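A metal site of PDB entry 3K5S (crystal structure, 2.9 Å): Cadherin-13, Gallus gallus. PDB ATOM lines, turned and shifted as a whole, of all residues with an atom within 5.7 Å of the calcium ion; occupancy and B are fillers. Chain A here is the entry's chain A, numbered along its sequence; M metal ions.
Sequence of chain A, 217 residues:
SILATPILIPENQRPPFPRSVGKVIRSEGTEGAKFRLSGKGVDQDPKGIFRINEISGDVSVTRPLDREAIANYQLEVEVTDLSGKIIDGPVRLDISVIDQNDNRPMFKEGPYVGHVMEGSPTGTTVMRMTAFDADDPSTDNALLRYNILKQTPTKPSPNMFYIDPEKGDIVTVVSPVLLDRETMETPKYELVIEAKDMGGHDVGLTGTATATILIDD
The backbone NH (N) of Asn 103 sits at hydrogen-bond distance from the side-chain carboxylate (OD2) of Asp 135, at 3.1 Å.
OD1 of Asp 102 lies close to ND2 of Asn 103 (3.1 Å).
The backbone NH of Asp 197 sits at hydrogen-bond distance from the backbone carbonyl oxygen of Leu 205, at 3.0 Å.
OD1 of Asn 101 lies close to OD2 of Asp 135 (3.0 Å).
The side-chain carboxylate (OD1) of Asp 133 lies close to the backbone NH (N) of Asp 135 (3.0 Å).
The calcium ion is bound by the backbone carbonyl oxygen (O) of Asn 103 (2.4 Å), the backbone carbonyl oxygen (O) of Asn 141 (2.5 Å), the side-chain carboxylate (OD2) of Asp 197 (2.6 Å), the side-chain amide oxygen (OD1) of Asn 101 (2.6 Å), the side-chain carboxylate (OD2) of Asp 133 (2.7 Å) and the side-chain carboxylate (OD1) of Asp 133 (2.7 Å).
The calcium ion has six donor atoms within binding distance.
Slightly farther from the calcium ion lies the side-chain carboxylate (OD2) of Asp 135 (3.1 Å).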
ATOM      1  N   ASN A 101      13.262 -21.602  21.283  1.00  0.00           N
ATOM      2  CA  ASN A 101      13.680 -22.950  20.893  1.00  0.00           C
ATOM      3  C   ASN A 101      13.237 -24.047  21.879  1.00  0.00           C
ATOM      4  O   ASN A 101      14.000 -24.469  22.734  1.00  0.00           O
ATOM      5  CB  ASN A 101      15.201 -22.987  20.705  1.00  0.00           C
ATOM      6  CG  ASN A 101      15.659 -24.199  19.912  1.00  0.00           C
ATOM      7  OD1 ASN A 101      14.990 -24.614  18.965  1.00  0.00           O
ATOM      8  ND2 ASN A 101      16.798 -24.777  20.295  1.00  0.00           N
ATOM      9  N   ASP A 102      12.005 -24.513  21.751  1.00  0.00           N
ATOM     10  CA  ASP A 102      11.473 -25.458  22.716  1.00  0.00           C
ATOM     11  C   ASP A 102      10.968 -26.741  22.105  1.00  0.00           C
ATOM     12  O   ASP A 102      10.247 -27.501  22.747  1.00  0.00           O
ATOM     13  CB  ASP A 102      10.392 -24.818  23.612  1.00  0.00           C
ATOM     14  CG  ASP A 102       9.213 -24.269  22.822  1.00  0.00           C
ATOM     15  OD1 ASP A 102       8.951 -24.748  21.701  1.00  0.00           O
ATOM     16  OD2 ASP A 102       8.544 -23.364  23.351  1.00  0.00           O
ATOM     17  N   ASN A 103      11.347 -26.988  20.873  1.00  0.00           N
ATOM     18  CA  ASN A 103      11.025 -28.263  20.269  1.00  0.00           C
ATOM     19  C   ASN A 103      12.292 -28.930  19.774  1.00  0.00           C
ATOM     20  O   ASN A 103      13.087 -28.308  19.099  1.00  0.00           O
ATOM     21  CB  ASN A 103      10.027 -28.101  19.131  1.00  0.00           C
ATOM     22  CG  ASN A 103       8.605 -27.993  19.622  1.00  0.00           C
ATOM     23  OD1 ASN A 103       8.015 -28.985  20.055  1.00  0.00           O
ATOM     24  ND2 ASN A 103       8.039 -26.798  19.542  1.00  0.00           N
ATOM     25  N   ARG A 104      12.489 -30.184  20.120  1.00  0.00           N
ATOM     26  CA  ARG A 104      13.734 -30.842  19.732  1.00  0.00           C
ATOM     27  C   ARG A 104      13.565 -31.470  18.345  1.00  0.00           C
ATOM     28  O   ARG A 104      12.513 -32.015  18.037  1.00  0.00           O
ATOM     29  CB  ARG A 104      14.113 -31.874  20.804  1.00  0.00           C
ATOM     30  CG  ARG A 104      15.008 -32.992  20.321  1.00  0.00           C
ATOM     31  CD  ARG A 104      14.849 -34.231  21.195  1.00  0.00           C
ATOM     32  NE  ARG A 104      14.609 -33.855  22.589  1.00  0.00           N
ATOM     33  CZ  ARG A 104      15.569 -33.510  23.439  1.00  0.00           C
ATOM     34  NH1 ARG A 104      16.841 -33.476  23.038  1.00  0.00           N
ATOM     35  NH2 ARG A 104      15.262 -33.179  24.699  1.00  0.00           N
ATOM     36  N   PRO A 105      14.602 -31.365  17.489  1.00  0.00           N
ATOM     37  CA  PRO A 105      14.579 -32.026  16.167  1.00  0.00           C
ATOM     38  C   PRO A 105      14.287 -33.523  16.286  1.00  0.00           C
ATOM     39  O   PRO A 105      14.866 -34.191  17.154  1.00  0.00           O
ATOM     40  CB  PRO A 105      16.021 -31.826  15.664  1.00  0.00           C
ATOM     41  CG  PRO A 105      16.563 -30.678  16.397  1.00  0.00           C
ATOM     42  CD  PRO A 105      15.867 -30.656  17.736  1.00  0.00           C
ATOM     43  N   ASP A 133      11.359 -30.386  12.677  1.00  0.00           N
ATOM     44  CA  ASP A 133      11.505 -29.577  13.889  1.00  0.00           C
ATOM     45  C   ASP A 133      10.319 -28.638  14.070  1.00  0.00           C
ATOM     46  O   ASP A 133      10.078 -27.768  13.246  1.00  0.00           O
ATOM     47  CB  ASP A 133      12.794 -28.757  13.814  1.00  0.00           C
ATOM     48  CG  ASP A 133      13.170 -28.162  15.144  1.00  0.00           C
ATOM     49  OD1 ASP A 133      12.346 -27.438  15.738  1.00  0.00           O
ATOM     50  OD2 ASP A 133      14.310 -28.424  15.603  1.00  0.00           O
ATOM     51  N   ALA A 134       9.589 -28.810  15.172  1.00  0.00           N
ATOM     52  CA  ALA A 134       8.349 -28.074  15.369  1.00  0.00           C
ATOM     53  C   ALA A 134       8.491 -26.548  15.421  1.00  0.00           C
ATOM     54  O   ALA A 134       7.499 -25.820  15.332  1.00  0.00           O
ATOM     55  CB  ALA A 134       7.608 -28.574  16.600  1.00  0.00           C
ATOM     56  N   ASP A 135       9.718 -26.060  15.555  1.00  0.00           N
ATOM     57  CA  ASP A 135       9.955 -24.623  15.727  1.00  0.00           C
ATOM     58  C   ASP A 135       9.939 -23.822  14.413  1.00  0.00           C
ATOM     59  O   ASP A 135       9.507 -24.331  13.381  1.00  0.00           O
ATOM     60  CB  ASP A 135      11.212 -24.379  16.556  1.00  0.00           C
ATOM     61  CG  ASP A 135      11.050 -24.851  17.999  1.00  0.00           C
ATOM     62  OD1 ASP A 135       9.963 -25.350  18.346  1.00  0.00           O
ATOM     63  OD2 ASP A 135      11.998 -24.734  18.795  1.00  0.00           O
ATOM     64  N   ASN A 141      15.910 -21.731  15.504  1.00  0.00           N
ATOM     65  CA  ASN A 141      15.361 -22.704  16.416  1.00  0.00           C
ATOM     66  C   ASN A 141      15.055 -23.997  15.674  1.00  0.00           C
ATOM     67  O   ASN A 141      15.265 -25.073  16.191  1.00  0.00           O
ATOM     68  CB  ASN A 141      14.198 -22.114  17.186  1.00  0.00           C
ATOM     69  CG  ASN A 141      14.585 -20.855  17.948  1.00  0.00           C
ATOM     70  OD1 ASN A 141      15.764 -20.521  18.045  1.00  0.00           O
ATOM     71  ND2 ASN A 141      13.602 -20.169  18.491  1.00  0.00           N
ATOM     72  N   ALA A 142      14.570 -23.878  14.443  1.00  0.00           N
ATOM     73  CA  ALA A 142      14.749 -24.926  13.453  1.00  0.00           C
ATOM     74  C   ALA A 142      15.915 -24.400  12.628  1.00  0.00           C
ATOM     75  O   ALA A 142      16.533 -23.439  13.035  1.00  0.00           O
ATOM     76  CB  ALA A 142      13.515 -25.104  12.613  1.00  0.00           C
ATOM     77  N   LEU A 144      18.424 -27.021  10.801  1.00  0.00           N
ATOM     78  CA  LEU A 144      19.129 -28.175  11.296  1.00  0.00           C
ATOM     79  C   LEU A 144      20.437 -28.421  10.527  1.00  0.00           C
ATOM     80  O   LEU A 144      20.562 -28.079   9.344  1.00  0.00           O
ATOM     81  CB  LEU A 144      18.205 -29.391  11.227  1.00  0.00           C
ATOM     82  CG  LEU A 144      16.725 -29.132  11.569  1.00  0.00           C
ATOM     83  CD1 LEU A 144      15.961 -30.445  11.695  1.00  0.00           C
ATOM     84  CD2 LEU A 144      16.517 -28.289  12.826  1.00  0.00           C
ATOM     85  N   ASP A 197      20.023 -28.452  16.115  1.00  0.00           N
ATOM     86  CA  ASP A 197      19.418 -27.121  16.005  1.00  0.00           C
ATOM     87  C   ASP A 197      20.436 -26.002  15.826  1.00  0.00           C
ATOM     88  O   ASP A 197      21.646 -26.233  15.845  1.00  0.00           O
ATOM     89  CB  ASP A 197      18.693 -26.799  17.301  1.00  0.00           C
ATOM     90  CG  ASP A 197      17.240 -27.008  17.207  1.00  0.00           C
ATOM     91  OD1 ASP A 197      16.774 -27.310  16.088  1.00  0.00           O
ATOM     92  OD2 ASP A 197      16.579 -26.857  18.244  1.00  0.00           O
ATOM     93  N   LEU A 205      19.884 -28.434  20.105  1.00  0.00           N
ATOM     94  CA  LEU A 205      19.205 -29.607  20.637  1.00  0.00           C
ATOM     95  C   LEU A 205      19.303 -30.674  19.561  1.00  0.00           C
ATOM     96  O   LEU A 205      19.466 -30.343  18.387  1.00  0.00           O
ATOM     97  CB  LEU A 205      17.738 -29.291  20.946  1.00  0.00           C
ATOM     98  CG  LEU A 205      17.437 -28.357  22.125  1.00  0.00           C
ATOM     99  CD1 LEU A 205      16.092 -27.682  21.926  1.00  0.00           C
ATOM    100  CD2 LEU A 205      17.508 -29.101  23.466  1.00  0.00           C
HETATM  101 CA    CA M   1      14.096 -26.682  17.653  1.00  0.00          CA
